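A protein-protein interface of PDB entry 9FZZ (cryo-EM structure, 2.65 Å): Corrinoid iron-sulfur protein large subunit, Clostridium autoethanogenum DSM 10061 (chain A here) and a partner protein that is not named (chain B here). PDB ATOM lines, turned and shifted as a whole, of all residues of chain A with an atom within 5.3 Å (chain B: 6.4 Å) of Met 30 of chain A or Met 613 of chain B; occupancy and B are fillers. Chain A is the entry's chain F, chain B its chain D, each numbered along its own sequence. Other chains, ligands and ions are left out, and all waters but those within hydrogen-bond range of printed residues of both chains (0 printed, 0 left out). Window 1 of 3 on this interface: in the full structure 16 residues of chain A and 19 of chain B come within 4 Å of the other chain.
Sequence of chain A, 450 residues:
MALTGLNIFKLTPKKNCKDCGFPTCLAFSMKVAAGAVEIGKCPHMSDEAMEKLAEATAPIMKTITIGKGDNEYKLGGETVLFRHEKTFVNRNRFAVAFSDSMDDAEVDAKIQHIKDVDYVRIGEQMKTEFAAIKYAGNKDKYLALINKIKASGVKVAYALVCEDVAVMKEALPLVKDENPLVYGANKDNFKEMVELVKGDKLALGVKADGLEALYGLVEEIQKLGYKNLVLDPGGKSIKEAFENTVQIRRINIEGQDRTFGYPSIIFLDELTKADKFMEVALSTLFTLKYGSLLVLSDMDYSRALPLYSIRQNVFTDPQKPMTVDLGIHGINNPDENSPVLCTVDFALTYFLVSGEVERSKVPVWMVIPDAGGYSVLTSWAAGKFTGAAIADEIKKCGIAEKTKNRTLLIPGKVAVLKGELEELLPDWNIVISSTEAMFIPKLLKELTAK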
ATOM      1  N   GLY A   5      19.367  20.853  13.538  1.00  0.00           N
ATOM      2  CA  GLY A   5      18.067  21.089  12.849  1.00  0.00           C
ATOM      3  C   GLY A   5      17.468  19.817  12.267  1.00  0.00           C
ATOM      4  O   GLY A   5      16.265  19.595  12.324  1.00  0.00           O
ATOM      5  N   LEU A   6      18.308  18.992  11.642  1.00  0.00           N
ATOM      6  CA  LEU A   6      17.845  17.690  11.174  1.00  0.00           C
ATOM      7  C   LEU A   6      17.114  16.927  12.278  1.00  0.00           C
ATOM      8  O   LEU A   6      16.114  16.219  12.020  1.00  0.00           O
ATOM      9  CB  LEU A   6      19.044  16.886  10.653  1.00  0.00           C
ATOM     10  CG  LEU A   6      18.839  16.231   9.283  1.00  0.00           C
ATOM     11  CD1 LEU A   6      18.787  17.283   8.171  1.00  0.00           C
ATOM     12  CD2 LEU A   6      19.937  15.217   9.010  1.00  0.00           C
ATOM     13  N   ILE A   8      15.190  18.288  14.704  1.00  0.00           N
ATOM     14  CA  ILE A   8      13.815  18.765  14.777  1.00  0.00           C
ATOM     15  C   ILE A   8      13.046  18.346  13.528  1.00  0.00           C
ATOM     16  O   ILE A   8      11.823  18.171  13.571  1.00  0.00           O
ATOM     17  CB  ILE A   8      13.792  20.277  15.019  1.00  0.00           C
ATOM     18  CG1 ILE A   8      14.452  21.005  13.865  1.00  0.00           C
ATOM     19  CG2 ILE A   8      14.566  20.605  16.292  1.00  0.00           C
ATOM     20  CD1 ILE A   8      14.277  22.453  13.939  1.00  0.00           C
ATOM     21  N   CYS A  25       9.317  21.222   4.843  1.00  0.00           N
ATOM     22  CA  CYS A  25       9.480  21.078   6.285  1.00  0.00           C
ATOM     23  C   CYS A  25      10.942  21.156   6.683  1.00  0.00           C
ATOM     24  O   CYS A  25      11.261  21.602   7.786  1.00  0.00           O
ATOM     25  CB  CYS A  25       8.892  19.745   6.764  1.00  0.00           C
ATOM     26  SG  CYS A  25       7.138  19.819   7.184  1.00  0.00           S
ATOM     27  N   LEU A  26      11.845  20.713   5.807  1.00  0.00           N
ATOM     28  CA  LEU A  26      13.266  20.849   6.097  1.00  0.00           C
ATOM     29  C   LEU A  26      13.668  22.315   6.166  1.00  0.00           C
ATOM     30  O   LEU A  26      14.465  22.711   7.021  1.00  0.00           O
ATOM     31  CB  LEU A  26      14.090  20.116   5.039  1.00  0.00           C
ATOM     32  CG  LEU A  26      15.576  19.934   5.381  1.00  0.00           C
ATOM     33  CD1 LEU A  26      15.807  18.620   6.119  1.00  0.00           C
ATOM     34  CD2 LEU A  26      16.412  20.002   4.111  1.00  0.00           C
ATOM     35  N   ALA A  27      13.127  23.139   5.266  1.00  0.00           N
ATOM     36  CA  ALA A  27      13.422  24.569   5.301  1.00  0.00           C
ATOM     37  C   ALA A  27      12.927  25.203   6.591  1.00  0.00           C
ATOM     38  O   ALA A  27      13.645  25.991   7.219  1.00  0.00           O
ATOM     39  CB  ALA A  27      12.804  25.262   4.085  1.00  0.00           C
ATOM     40  N   PHE A  28      11.716  24.851   7.015  1.00  0.00           N
ATOM     41  CA  PHE A  28      11.194  25.362   8.280  1.00  0.00           C
ATOM     42  C   PHE A  28      12.050  24.892   9.448  1.00  0.00           C
ATOM     43  O   PHE A  28      12.356  25.671  10.361  1.00  0.00           O
ATOM     44  CB  PHE A  28       9.735  24.924   8.452  1.00  0.00           C
ATOM     45  CG  PHE A  28       9.177  25.179   9.826  1.00  0.00           C
ATOM     46  CD1 PHE A  28       8.697  26.444  10.172  1.00  0.00           C
ATOM     47  CD2 PHE A  28       9.135  24.157  10.775  1.00  0.00           C
ATOM     48  CE1 PHE A  28       8.182  26.698  11.455  1.00  0.00           C
ATOM     49  CE2 PHE A  28       8.626  24.384  12.064  1.00  0.00           C
ATOM     50  CZ  PHE A  28       8.146  25.661  12.406  1.00  0.00           C
ATOM     51  N   SER A  29      12.458  23.624   9.430  1.00  0.00           N
ATOM     52  CA  SER A  29      13.284  23.084  10.503  1.00  0.00           C
ATOM     53  C   SER A  29      14.620  23.809  10.580  1.00  0.00           C
ATOM     54  O   SER A  29      15.088  24.154  11.670  1.00  0.00           O
ATOM     55  CB  SER A  29      13.470  21.578  10.267  1.00  0.00           C
ATOM     56  OG  SER A  29      14.594  21.059  10.967  1.00  0.00           O
ATOM     57  N   MET A  30      15.214  24.130   9.438  1.00  0.00           N
ATOM     58  CA  MET A  30      16.479  24.857   9.471  1.00  0.00           C
ATOM     59  C   MET A  30      16.281  26.312   9.882  1.00  0.00           C
ATOM     60  O   MET A  30      17.136  26.882  10.569  1.00  0.00           O
ATOM     61  CB  MET A  30      17.171  24.763   8.108  1.00  0.00           C
ATOM     62  CG  MET A  30      17.587  23.324   7.754  1.00  0.00           C
ATOM     63  SD  MET A  30      18.804  22.654   8.904  1.00  0.00           S
ATOM     64  CE  MET A  30      18.735  20.907   8.541  1.00  0.00           C
ATOM     65  N   LYS A  31      15.161  26.924   9.498  1.00  0.00           N
ATOM     66  CA  LYS A  31      14.897  28.295   9.926  1.00  0.00           C
ATOM     67  C   LYS A  31      14.707  28.386  11.435  1.00  0.00           C
ATOM     68  O   LYS A  31      15.204  29.322  12.071  1.00  0.00           O
ATOM     69  CB  LYS A  31      13.667  28.844   9.195  1.00  0.00           C
ATOM     70  CG  LYS A  31      13.895  29.083   7.687  1.00  0.00           C
ATOM     71  CD  LYS A  31      15.069  30.058   7.426  1.00  0.00           C
ATOM     72  CE  LYS A  31      14.756  31.471   7.953  1.00  0.00           C
ATOM     73  NZ  LYS A  31      13.592  32.072   7.213  1.00  0.00           N
ATOM     74  N   VAL A  32      13.992  27.431  12.033  1.00  0.00           N
ATOM     75  CA  VAL A  32      13.844  27.449  13.487  1.00  0.00           C
ATOM     76  C   VAL A  32      15.097  26.940  14.192  1.00  0.00           C
ATOM     77  O   VAL A  32      15.297  27.235  15.375  1.00  0.00           O
ATOM     78  CB  VAL A  32      12.616  26.648  13.948  1.00  0.00           C
ATOM     79  CG1 VAL A  32      11.371  27.071  13.161  1.00  0.00           C
ATOM     80  CG2 VAL A  32      12.860  25.165  13.810  1.00  0.00           C
ATOM     81  N   ALA A  33      15.950  26.179  13.496  1.00  0.00           N
ATOM     82  CA  ALA A  33      17.206  25.742  14.099  1.00  0.00           C
ATOM     83  C   ALA A  33      18.139  26.920  14.333  1.00  0.00           C
ATOM     84  O   ALA A  33      18.833  26.977  15.353  1.00  0.00           O
ATOM     85  CB  ALA A  33      17.882  24.692  13.211  1.00  0.00           C
ATOM     86  N   ALA A  34      18.174  27.866  13.397  1.00  0.00           N
ATOM     87  CA  ALA A  34      19.024  29.038  13.544  1.00  0.00           C
ATOM     88  C   ALA A  34      18.500  30.015  14.586  1.00  0.00           C
ATOM     89  O   ALA A  34      19.211  30.962  14.933  1.00  0.00           O
ATOM     90  CB  ALA A  34      19.172  29.753  12.196  1.00  0.00           C
ATOM     91  N   MET B 605      15.492  25.664  -0.284  1.00  0.00           N
ATOM     92  CA  MET B 605      16.389  26.770   0.001  1.00  0.00           C
ATOM     93  C   MET B 605      17.270  27.022  -1.215  1.00  0.00           C
ATOM     94  O   MET B 605      17.568  26.107  -1.988  1.00  0.00           O
ATOM     95  CB  MET B 605      17.260  26.483   1.229  1.00  0.00           C
ATOM     96  CG  MET B 605      16.534  25.648   2.287  1.00  0.00           C
ATOM     97  SD  MET B 605      17.638  25.178   3.630  1.00  0.00           S
ATOM     98  CE  MET B 605      16.939  23.619   4.136  1.00  0.00           C
ATOM     99  N   GLY B 608      22.282  30.634  -1.402  1.00  0.00           N
ATOM    100  CA  GLY B 608      22.702  31.547  -0.351  1.00  0.00           C
ATOM    101  C   GLY B 608      22.350  31.040   1.033  1.00  0.00           C
ATOM    102  O   GLY B 608      23.170  31.081   1.954  1.00  0.00           O
ATOM    103  N   GLU B 609      21.121  30.553   1.202  1.00  0.00           N
ATOM    104  CA  GLU B 609      20.704  30.027   2.501  1.00  0.00           C
ATOM    105  C   GLU B 609      21.492  28.776   2.871  1.00  0.00           C
ATOM    106  O   GLU B 609      21.888  28.601   4.030  1.00  0.00           O
ATOM    107  CB  GLU B 609      19.203  29.742   2.491  1.00  0.00           C
ATOM    108  CG  GLU B 609      18.367  31.008   2.287  1.00  0.00           C
ATOM    109  CD  GLU B 609      16.877  30.720   2.216  1.00  0.00           C
ATOM    110  OE1 GLU B 609      16.512  29.537   2.093  1.00  0.00           O
ATOM    111  OE2 GLU B 609      16.076  31.675   2.288  1.00  0.00           O
ATOM    112  N   LEU B 610      21.732  27.898   1.900  1.00  0.00           N
ATOM    113  CA  LEU B 610      22.523  26.701   2.170  1.00  0.00           C
ATOM    114  C   LEU B 610      23.953  27.064   2.540  1.00  0.00           C
ATOM    115  O   LEU B 610      24.553  26.438   3.417  1.00  0.00           O
ATOM    116  CB  LEU B 610      22.491  25.767   0.958  1.00  0.00           C
ATOM    117  CG  LEU B 610      21.130  25.115   0.666  1.00  0.00           C
ATOM    118  CD1 LEU B 610      21.231  24.205  -0.546  1.00  0.00           C
ATOM    119  CD2 LEU B 610      20.626  24.327   1.863  1.00  0.00           C
ATOM    120  N   ALA B 611      24.519  28.068   1.876  1.00  0.00           N
ATOM    121  CA  ALA B 611      25.869  28.511   2.209  1.00  0.00           C
ATOM    122  C   ALA B 611      25.919  29.131   3.599  1.00  0.00           C
ATOM    123  O   ALA B 611      26.889  28.928   4.338  1.00  0.00           O
ATOM    124  CB  ALA B 611      26.375  29.498   1.156  1.00  0.00           C
ATOM    125  N   SER B 612      24.894  29.902   3.969  1.00  0.00           N
ATOM    126  CA  SER B 612      24.854  30.477   5.312  1.00  0.00           C
ATOM    127  C   SER B 612      24.733  29.392   6.371  1.00  0.00           C
ATOM    128  O   SER B 612      25.337  29.491   7.444  1.00  0.00           O
ATOM    129  CB  SER B 612      23.680  31.455   5.444  1.00  0.00           C
ATOM    130  OG  SER B 612      23.826  32.568   4.570  1.00  0.00           O
ATOM    131  N   MET B 613      23.945  28.358   6.094  1.00  0.00           N
ATOM    132  CA  MET B 613      23.751  27.291   7.068  1.00  0.00           C
ATOM    133  C   MET B 613      24.951  26.356   7.161  1.00  0.00           C
ATOM    134  O   MET B 613      25.232  25.828   8.240  1.00  0.00           O
ATOM    135  CB  MET B 613      22.495  26.500   6.712  1.00  0.00           C
ATOM    136  CG  MET B 613      22.064  25.512   7.784  1.00  0.00           C
ATOM    137  SD  MET B 613      21.514  23.955   7.047  1.00  0.00           S
ATOM    138  CE  MET B 613      20.488  24.506   5.681  1.00  0.00           C
ATOM    139  N   THR B 614      25.663  26.136   6.053  1.00  0.00           N
ATOM    140  CA  THR B 614      26.698  25.113   5.974  1.00  0.00           C
ATOM    141  C   THR B 614      28.086  25.638   6.313  1.00  0.00           C
ATOM    142  O   THR B 614      28.841  24.969   7.022  1.00  0.00           O
ATOM    143  CB  THR B 614      26.726  24.518   4.559  1.00  0.00           C
ATOM    144  OG1 THR B 614      25.452  23.951   4.231  1.00  0.00           O
ATOM    145  CG2 THR B 614      27.782  23.441   4.446  1.00  0.00           C
ATOM    146  N   GLY B 615      28.443  26.816   5.809  1.00  0.00           N
ATOM    147  CA  GLY B 615      29.779  27.339   5.981  1.00  0.00           C
ATOM    148  C   GLY B 615      30.025  27.892   7.370  1.00  0.00           C
ATOM    149  O   GLY B 615      29.170  27.860   8.257  1.00  0.00           O
ATOM    150  N   VAL B 618      31.403  25.060  10.899  1.00  0.00           N
ATOM    151  CA  VAL B 618      30.490  24.414  11.832  1.00  0.00           C
ATOM    152  C   VAL B 618      30.107  23.052  11.271  1.00  0.00           C
ATOM    153  O   VAL B 618      29.850  22.916  10.068  1.00  0.00           O
ATOM    154  CB  VAL B 618      29.246  25.287  12.098  1.00  0.00           C
ATOM    155  CG1 VAL B 618      28.586  25.714  10.790  1.00  0.00           C
ATOM    156  CG2 VAL B 618      28.250  24.548  12.988  1.00  0.00           C
ATOM    157  N   THR B 620      27.677  20.576  10.430  1.00  0.00           N
ATOM    158  CA  THR B 620      26.238  20.486  10.177  1.00  0.00           C
ATOM    159  C   THR B 620      25.934  19.161   9.493  1.00  0.00           C
ATOM    160  O   THR B 620      26.156  19.020   8.277  1.00  0.00           O
ATOM    161  CB  THR B 620      25.748  21.656   9.322  1.00  0.00           C
ATOM    162  OG1 THR B 620      26.328  21.599   8.012  1.00  0.00           O
ATOM    163  CG2 THR B 620      26.129  22.973   9.967  1.00  0.00           C
ATOM    164  N   PRO B 621      25.440  18.153  10.220  1.00  0.00           N
ATOM    165  CA  PRO B 621      25.112  16.877   9.570  1.00  0.00           C
ATOM    166  C   PRO B 621      24.037  17.057   8.510  1.00  0.00           C
ATOM    167  O   PRO B 621      23.078  17.812   8.685  1.00  0.00           O
ATOM    168  CB  PRO B 621      24.634  15.992  10.728  1.00  0.00           C
ATOM    169  CG  PRO B 621      25.263  16.610  11.969  1.00  0.00           C
ATOM    170  CD  PRO B 621      25.272  18.092  11.683  1.00  0.00           C
ATOM    171  N   PHE B 623      24.564  18.292   5.454  1.00  0.00           N
ATOM    172  CA  PHE B 623      24.934  19.287   4.455  1.00  0.00           C
ATOM    173  C   PHE B 623      26.447  19.360   4.355  1.00  0.00           C
ATOM    174  O   PHE B 623      27.148  19.266   5.364  1.00  0.00           O
ATOM    175  CB  PHE B 623      24.350  20.663   4.790  1.00  0.00           C
ATOM    176  CG  PHE B 623      22.863  20.719   4.659  1.00  0.00           C
ATOM    177  CD1 PHE B 623      22.050  20.354   5.724  1.00  0.00           C
ATOM    178  CD2 PHE B 623      22.273  21.096   3.455  1.00  0.00           C
ATOM    179  CE1 PHE B 623      20.663  20.378   5.604  1.00  0.00           C
ATOM    180  CE2 PHE B 623      20.882  21.128   3.314  1.00  0.00           C
ATOM    181  CZ  PHE B 623      20.074  20.767   4.395  1.00  0.00           C
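The side-chain sulfur of Met 613 of chain B lies close to the side-chain sulfur of Met 30 of chain A.
CE of Met 605 of chain B touches CD2 of Leu 26 of chain A (3.7 Å).
Phe 623 of chain B touches Leu 26 of chain A (CZ to CD2, 3.8 Å).
Met 605 of chain B touches Ala 27 of chain A (CE to CA, 3.8 Å).
Met 30 of chain A touches Met 605 of chain B.
CE1 of Phe 623 of chain B touches CE of Met 30 of chain A, 3.6 Å away.
Met 613 of chain B touches one residue of chain A.
Printed residues of chain A within 4 Å of Met 605 of chain B: Leu 26, Ala 27 and Met 30.
Printed residues of chain A within 4 Å of Phe 623 of chain B: Leu 26 and Met 30.
Of the printed residues of chain B, Ala 27 of chain A touches Met 605 (3.8 Å).
The nearest printed residue of chain A that does not touch Met 613 of chain B is Leu 26 of chain A (6.3 Å).
Hydrophobic or aromatic side chains of chain A within 4 Å of the printed part of chain B: Leu 26 and Met 30.
Of the 13 printed residues of chain B, 3 touch a printed residue of chain A.
Among the printed residues, 6 pairs touch across the chains.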
